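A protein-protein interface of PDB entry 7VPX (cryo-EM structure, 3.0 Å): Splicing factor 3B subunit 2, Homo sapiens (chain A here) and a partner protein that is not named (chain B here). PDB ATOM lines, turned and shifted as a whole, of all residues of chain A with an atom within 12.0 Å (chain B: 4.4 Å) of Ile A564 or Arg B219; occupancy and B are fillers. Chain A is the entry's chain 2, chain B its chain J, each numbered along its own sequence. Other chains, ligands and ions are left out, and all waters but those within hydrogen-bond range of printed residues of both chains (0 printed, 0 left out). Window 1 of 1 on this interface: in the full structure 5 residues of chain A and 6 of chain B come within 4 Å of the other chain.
Ile A564 touches Phe B212. CD of Arg B219 touches O of Ile A564, 3.6 Å away. O of Ile A566 touches OG of Ser B222, at 3.6 Å. Trp B223 touches Tyr A568.
The backbone carbonyl oxygen (O) of Phe B212 is in hydrogen-bond range of the guanidinium group (NH1) of Arg B219, at 2.9 Å. The guanidinium group (NH1) of Arg B219 lies close to the backbone carbonyl oxygen (O) of Ser B215 (3.5 Å).
Printed residues of chain B that touch a printed residue of chain A: Phe B212, Ser B215, Arg B219, Ser B222 and Trp B223. Along chain B the printed residues that touch a printed residue of chain A span positions 212 to 223. Hydrophobic or aromatic side chains of chain A within 4 Å of the printed part of chain B: Ile A564 and Tyr A568. Among the printed residues, no Asp or Glu carboxylate lies within 4 Å of a Lys or Arg side-chain nitrogen of the other chain.
Gln A534 touches none of the printed residues of chain B. Of chain B, only Phe B212 (3.9 Å), Ser B215 (2.9 Å) and Arg B219 (3.6 Å) come within 4 Å of Ile A564. Printed residues of chain B within 4 Å of Ile A566: Ser B222 (3.6 Å). Of the printed residues of chain B, Tyr A568 touches Trp B223. Leu A571 touches none of the printed residues of chain B. Printed residues of chain A within 4 Å of Ser B215: Ile A564. No residue of chain A comes within 4 Å of Arg B216. No residue of chain A comes within 4 Å of Gly B218. Arg B219 touches just one residue of chain A: Ile A564. No residue of chain A comes within 4 Å of Val B220. Of the printed residues of chain A, Trp B223 touches Tyr A568 (3.1 Å). The nearest printed residue of chain B that does not touch Ile A564 is Arg B216 (6.3 Å).
The side-chain hydroxyl (OG) of Ser B215 lies within hydrogen-bond range of the backbone NH (N) of Ile A564 (2.9 Å).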
ATOM      1  N   THR A 531      -6.355   5.899 -13.292  1.00  0.00           N
ATOM      2  CA  THR A 531      -4.925   5.564 -13.015  1.00  0.00           C
ATOM      3  C   THR A 531      -4.777   4.739 -11.726  1.00  0.00           C
ATOM      4  O   THR A 531      -3.685   4.177 -11.515  1.00  0.00           O
ATOM      5  CB  THR A 531      -4.046   6.821 -12.956  1.00  0.00           C
ATOM      6  OG1 THR A 531      -2.906   6.604 -13.789  1.00  0.00           O
ATOM      7  CG2 THR A 531      -3.597   7.159 -11.551  1.00  0.00           C
ATOM      8  N   GLY A 532      -5.823   4.692 -10.896  1.00  0.00           N
ATOM      9  CA  GLY A 532      -5.838   3.916  -9.641  1.00  0.00           C
ATOM     10  C   GLY A 532      -4.902   4.502  -8.597  1.00  0.00           C
ATOM     11  O   GLY A 532      -4.191   3.720  -7.937  1.00  0.00           O
ATOM     12  N   ILE A 533      -4.880   5.833  -8.477  1.00  0.00           N
ATOM     13  CA  ILE A 533      -4.152   6.509  -7.361  1.00  0.00           C
ATOM     14  C   ILE A 533      -5.073   6.568  -6.137  1.00  0.00           C
ATOM     15  O   ILE A 533      -6.207   7.068  -6.274  1.00  0.00           O
ATOM     16  CB  ILE A 533      -3.675   7.914  -7.783  1.00  0.00           C
ATOM     17  CG1 ILE A 533      -2.617   7.845  -8.887  1.00  0.00           C
ATOM     18  CG2 ILE A 533      -3.179   8.698  -6.579  1.00  0.00           C
ATOM     19  CD1 ILE A 533      -2.097   9.194  -9.323  1.00  0.00           C
ATOM     20  N   GLN A 534      -4.582   6.095  -4.987  1.00  0.00           N
ATOM     21  CA  GLN A 534      -5.362   6.094  -3.719  1.00  0.00           C
ATOM     22  C   GLN A 534      -4.395   6.204  -2.535  1.00  0.00           C
ATOM     23  O   GLN A 534      -4.501   7.209  -1.804  1.00  0.00           O
ATOM     24  CB  GLN A 534      -6.213   4.827  -3.608  1.00  0.00           C
ATOM     25  CG  GLN A 534      -7.572   4.941  -4.283  1.00  0.00           C
ATOM     26  CD  GLN A 534      -8.429   3.722  -4.045  1.00  0.00           C
ATOM     27  OE1 GLN A 534      -7.945   2.670  -3.631  1.00  0.00           O
ATOM     28  NE2 GLN A 534      -9.718   3.857  -4.307  1.00  0.00           N
ATOM     29  N   ILE A 564       3.586  -1.880  -2.613  1.00  0.00           N
ATOM     30  CA  ILE A 564       2.839  -1.038  -3.595  1.00  0.00           C
ATOM     31  C   ILE A 564       3.631  -0.985  -4.906  1.00  0.00           C
ATOM     32  O   ILE A 564       4.822  -0.618  -4.864  1.00  0.00           O
ATOM     33  CB  ILE A 564       2.579   0.373  -3.026  1.00  0.00           C
ATOM     34  CG1 ILE A 564       1.737   1.222  -3.982  1.00  0.00           C
ATOM     35  CG2 ILE A 564       3.887   1.059  -2.666  1.00  0.00           C
ATOM     36  CD1 ILE A 564       1.426   2.606  -3.463  1.00  0.00           C
ATOM     37  N   ASP A 565       2.981  -1.327  -6.023  1.00  0.00           N
ATOM     38  CA  ASP A 565       3.636  -1.318  -7.359  1.00  0.00           C
ATOM     39  C   ASP A 565       3.031  -0.185  -8.195  1.00  0.00           C
ATOM     40  O   ASP A 565       1.792  -0.136  -8.315  1.00  0.00           O
ATOM     41  CB  ASP A 565       3.488  -2.675  -8.054  1.00  0.00           C
ATOM     42  CG  ASP A 565       4.154  -3.815  -7.303  1.00  0.00           C
ATOM     43  OD1 ASP A 565       4.943  -3.528  -6.382  1.00  0.00           O
ATOM     44  OD2 ASP A 565       3.879  -4.982  -7.648  1.00  0.00           O
ATOM     45  N   ILE A 566       3.883   0.675  -8.762  1.00  0.00           N
ATOM     46  CA  ILE A 566       3.415   1.831  -9.582  1.00  0.00           C
ATOM     47  C   ILE A 566       3.964   1.701 -11.007  1.00  0.00           C
ATOM     48  O   ILE A 566       5.176   1.451 -11.153  1.00  0.00           O
ATOM     49  CB  ILE A 566       3.829   3.167  -8.933  1.00  0.00           C
ATOM     50  CG1 ILE A 566       5.344   3.380  -8.992  1.00  0.00           C
ATOM     51  CG2 ILE A 566       3.300   3.260  -7.511  1.00  0.00           C
ATOM     52  CD1 ILE A 566       5.797   4.714  -8.447  1.00  0.00           C
ATOM     53  N   ASP A 567       3.099   1.884 -12.011  1.00  0.00           N
ATOM     54  CA  ASP A 567       3.511   1.804 -13.438  1.00  0.00           C
ATOM     55  C   ASP A 567       3.644   3.230 -13.980  1.00  0.00           C
ATOM     56  O   ASP A 567       2.667   3.995 -13.872  1.00  0.00           O
ATOM     57  CB  ASP A 567       2.498   1.006 -14.264  1.00  0.00           C
ATOM     58  CG  ASP A 567       2.288  -0.416 -13.774  1.00  0.00           C
ATOM     59  OD1 ASP A 567       2.916  -0.786 -12.762  1.00  0.00           O
ATOM     60  OD2 ASP A 567       1.500  -1.143 -14.409  1.00  0.00           O
ATOM     61  N   TYR A 568       4.806   3.562 -14.551  1.00  0.00           N
ATOM     62  CA  TYR A 568       5.056   4.924 -15.094  1.00  0.00           C
ATOM     63  C   TYR A 568       4.511   5.028 -16.522  1.00  0.00           C
ATOM     64  O   TYR A 568       3.754   5.979 -16.799  1.00  0.00           O
ATOM     65  CB  TYR A 568       6.548   5.258 -15.026  1.00  0.00           C
ATOM     66  CG  TYR A 568       7.062   5.532 -13.635  1.00  0.00           C
ATOM     67  CD1 TYR A 568       7.167   6.825 -13.154  1.00  0.00           C
ATOM     68  CD2 TYR A 568       7.433   4.496 -12.795  1.00  0.00           C
ATOM     69  CE1 TYR A 568       7.635   7.084 -11.875  1.00  0.00           C
ATOM     70  CE2 TYR A 568       7.901   4.736 -11.514  1.00  0.00           C
ATOM     71  CZ  TYR A 568       8.002   6.036 -11.052  1.00  0.00           C
ATOM     72  OH  TYR A 568       8.463   6.282  -9.792  1.00  0.00           O
ATOM     73  N   GLN A 569       4.884   4.075 -17.384  1.00  0.00           N
ATOM     74  CA  GLN A 569       4.436   4.052 -18.802  1.00  0.00           C
ATOM     75  C   GLN A 569       2.913   4.205 -18.842  1.00  0.00           C
ATOM     76  O   GLN A 569       2.419   4.976 -19.688  1.00  0.00           O
ATOM     77  CB  GLN A 569       4.855   2.737 -19.464  1.00  0.00           C
ATOM     78  CG  GLN A 569       4.315   2.573 -20.877  1.00  0.00           C
ATOM     79  CD  GLN A 569       4.628   3.764 -21.749  1.00  0.00           C
ATOM     80  OE1 GLN A 569       5.202   4.753 -21.300  1.00  0.00           O
ATOM     81  NE2 GLN A 569       4.247   3.679 -23.013  1.00  0.00           N
ATOM     82  N   LYS A 570       2.209   3.524 -17.933  1.00  0.00           N
ATOM     83  CA  LYS A 570       0.727   3.608 -17.860  1.00  0.00           C
ATOM     84  C   LYS A 570       0.341   5.056 -17.540  1.00  0.00           C
ATOM     85  O   LYS A 570      -0.596   5.574 -18.176  1.00  0.00           O
ATOM     86  CB  LYS A 570       0.223   2.657 -16.769  1.00  0.00           C
ATOM     87  CG  LYS A 570      -1.273   2.694 -16.495  1.00  0.00           C
ATOM     88  CD  LYS A 570      -1.686   1.738 -15.396  1.00  0.00           C
ATOM     89  CE  LYS A 570      -3.169   1.767 -15.095  1.00  0.00           C
ATOM     90  NZ  LYS A 570      -3.527   0.816 -14.017  1.00  0.00           N
ATOM     91  N   LEU A 571       1.070   5.684 -16.612  1.00  0.00           N
ATOM     92  CA  LEU A 571       0.817   7.094 -16.209  1.00  0.00           C
ATOM     93  C   LEU A 571       1.067   8.026 -17.400  1.00  0.00           C
ATOM     94  O   LEU A 571       0.252   8.944 -17.611  1.00  0.00           O
ATOM     95  CB  LEU A 571       1.747   7.435 -15.039  1.00  0.00           C
ATOM     96  CG  LEU A 571       1.593   8.841 -14.463  1.00  0.00           C
ATOM     97  CD1 LEU A 571       2.371   8.981 -13.164  1.00  0.00           C
ATOM     98  CD2 LEU A 571       2.040   9.891 -15.468  1.00  0.00           C
ATOM     99  N   PHE B 212       6.151   0.105   1.915  1.00  0.00           N
ATOM    100  CA  PHE B 212       6.740   1.119   1.006  1.00  0.00           C
ATOM    101  C   PHE B 212       8.245   0.875   0.867  1.00  0.00           C
ATOM    102  O   PHE B 212       8.753   0.928  -0.271  1.00  0.00           O
ATOM    103  CB  PHE B 212       6.459   2.518   1.562  1.00  0.00           C
ATOM    104  CG  PHE B 212       6.526   3.636   0.551  1.00  0.00           C
ATOM    105  CD1 PHE B 212       7.607   4.502   0.519  1.00  0.00           C
ATOM    106  CD2 PHE B 212       5.503   3.827  -0.364  1.00  0.00           C
ATOM    107  CE1 PHE B 212       7.666   5.530  -0.409  1.00  0.00           C
ATOM    108  CE2 PHE B 212       5.563   4.854  -1.292  1.00  0.00           C
ATOM    109  CZ  PHE B 212       6.645   5.704  -1.313  1.00  0.00           C
ATOM    110  N   SER B 215       8.891  -2.600  -0.764  1.00  0.00           N
ATOM    111  CA  SER B 215       8.539  -2.373  -2.174  1.00  0.00           C
ATOM    112  C   SER B 215       9.474  -1.385  -2.894  1.00  0.00           C
ATOM    113  O   SER B 215       9.195  -0.993  -4.030  1.00  0.00           O
ATOM    114  CB  SER B 215       7.093  -1.885  -2.297  1.00  0.00           C
ATOM    115  OG  SER B 215       6.184  -2.794  -1.718  1.00  0.00           O
ATOM    116  N   ARG B 216      10.475  -0.875  -2.165  1.00  0.00           N
ATOM    117  CA  ARG B 216      11.358   0.227  -2.653  1.00  0.00           C
ATOM    118  C   ARG B 216      12.263  -0.178  -3.823  1.00  0.00           C
ATOM    119  O   ARG B 216      12.225   0.521  -4.864  1.00  0.00           O
ATOM    120  CB  ARG B 216      12.182   0.810  -1.499  1.00  0.00           C
ATOM    121  CG  ARG B 216      12.648   2.237  -1.746  1.00  0.00           C
ATOM    122  CD  ARG B 216      13.400   2.836  -0.574  1.00  0.00           C
ATOM    123  NE  ARG B 216      13.516   4.282  -0.684  1.00  0.00           N
ATOM    124  CZ  ARG B 216      14.275   5.038   0.102  1.00  0.00           C
ATOM    125  NH1 ARG B 216      14.312   6.348  -0.074  1.00  0.00           N
ATOM    126  NH2 ARG B 216      14.995   4.483   1.059  1.00  0.00           N
ATOM    127  N   ASP B 217      13.035  -1.257  -3.675  1.00  0.00           N
ATOM    128  CA  ASP B 217      13.979  -1.650  -4.756  1.00  0.00           C
ATOM    129  C   ASP B 217      13.193  -1.944  -6.037  1.00  0.00           C
ATOM    130  O   ASP B 217      13.600  -1.441  -7.104  1.00  0.00           O
ATOM    131  CB  ASP B 217      14.855  -2.827  -4.319  1.00  0.00           C
ATOM    132  CG  ASP B 217      15.868  -2.450  -3.254  1.00  0.00           C
ATOM    133  OD1 ASP B 217      15.716  -1.362  -2.664  1.00  0.00           O
ATOM    134  OD2 ASP B 217      16.803  -3.242  -3.025  1.00  0.00           O
ATOM    135  N   GLY B 218      12.063  -2.648  -5.922  1.00  0.00           N
ATOM    136  CA  GLY B 218      11.265  -2.968  -7.119  1.00  0.00           C
ATOM    137  C   GLY B 218      10.773  -1.706  -7.806  1.00  0.00           C
ATOM    138  O   GLY B 218      10.916  -1.618  -9.038  1.00  0.00           O
ATOM    139  N   ARG B 219      10.282  -0.734  -7.031  1.00  0.00           N
ATOM    140  CA  ARG B 219       9.776   0.541  -7.609  1.00  0.00           C
ATOM    141  C   ARG B 219      10.922   1.284  -8.307  1.00  0.00           C
ATOM    142  O   ARG B 219      10.695   1.791  -9.425  1.00  0.00           O
ATOM    143  CB  ARG B 219       9.153   1.418  -6.521  1.00  0.00           C
ATOM    144  CG  ARG B 219       7.751   0.995  -6.106  1.00  0.00           C
ATOM    145  CD  ARG B 219       6.995   2.141  -5.462  1.00  0.00           C
ATOM    146  NE  ARG B 219       7.880   2.964  -4.653  1.00  0.00           N
ATOM    147  CZ  ARG B 219       8.123   2.765  -3.365  1.00  0.00           C
ATOM    148  NH1 ARG B 219       7.544   1.762  -2.728  1.00  0.00           N
ATOM    149  NH2 ARG B 219       8.946   3.570  -2.718  1.00  0.00           N
ATOM    150  N   VAL B 220      12.108   1.318  -7.688  1.00  0.00           N
ATOM    151  CA  VAL B 220      13.261   2.034  -8.316  1.00  0.00           C
ATOM    152  C   VAL B 220      13.607   1.342  -9.639  1.00  0.00           C
ATOM    153  O   VAL B 220      13.815   2.053 -10.654  1.00  0.00           O
ATOM    154  CB  VAL B 220      14.477   2.077  -7.373  1.00  0.00           C
ATOM    155  CG1 VAL B 220      15.684   2.711  -8.047  1.00  0.00           C
ATOM    156  CG2 VAL B 220      14.155   2.796  -6.073  1.00  0.00           C
ATOM    157  N   ASP B 221      13.602   0.004  -9.638  1.00  0.00           N
ATOM    158  CA  ASP B 221      13.934  -0.769 -10.864  1.00  0.00           C
ATOM    159  C   ASP B 221      12.896  -0.448 -11.943  1.00  0.00           C
ATOM    160  O   ASP B 221      13.298  -0.215 -13.096  1.00  0.00           O
ATOM    161  CB  ASP B 221      14.000  -2.268 -10.567  1.00  0.00           C
ATOM    162  CG  ASP B 221      15.281  -2.689  -9.865  1.00  0.00           C
ATOM    163  OD1 ASP B 221      16.275  -1.942  -9.965  1.00  0.00           O
ATOM    164  OD2 ASP B 221      15.275  -3.758  -9.225  1.00  0.00           O
ATOM    165  N   SER B 222      11.620  -0.374 -11.555  1.00  0.00           N
ATOM    166  CA  SER B 222      10.524  -0.071 -12.510  1.00  0.00           C
ATOM    167  C   SER B 222      10.735   1.322 -13.108  1.00  0.00           C
ATOM    168  O   SER B 222      10.615   1.459 -14.341  1.00  0.00           O
ATOM    169  CB  SER B 222       9.186  -0.168 -11.825  1.00  0.00           C
ATOM    170  OG  SER B 222       8.147   0.260 -12.693  1.00  0.00           O
ATOM    171  N   TRP B 223      11.097   2.302 -12.273  1.00  0.00           N
ATOM    172  CA  TRP B 223      11.323   3.678 -12.789  1.00  0.00           C
ATOM    173  C   TRP B 223      12.488   3.661 -13.782  1.00  0.00           C
ATOM    174  O   TRP B 223      12.351   4.272 -14.861  1.00  0.00           O
ATOM    175  CB  TRP B 223      11.596   4.659 -11.644  1.00  0.00           C
ATOM    176  CG  TRP B 223      12.241   5.929 -12.109  1.00  0.00           C
ATOM    177  CD1 TRP B 223      13.535   6.312 -11.916  1.00  0.00           C
ATOM    178  CD2 TRP B 223      11.626   6.979 -12.876  1.00  0.00           C
ATOM    179  NE1 TRP B 223      13.764   7.531 -12.495  1.00  0.00           N
ATOM    180  CE2 TRP B 223      12.612   7.965 -13.094  1.00  0.00           C
ATOM    181  CE3 TRP B 223      10.341   7.188 -13.392  1.00  0.00           C
ATOM    182  CZ2 TRP B 223      12.350   9.134 -13.804  1.00  0.00           C
ATOM    183  CZ3 TRP B 223      10.084   8.344 -14.094  1.00  0.00           C
ATOM    184  CH2 TRP B 223      11.076   9.303 -14.295  1.00  0.00           C
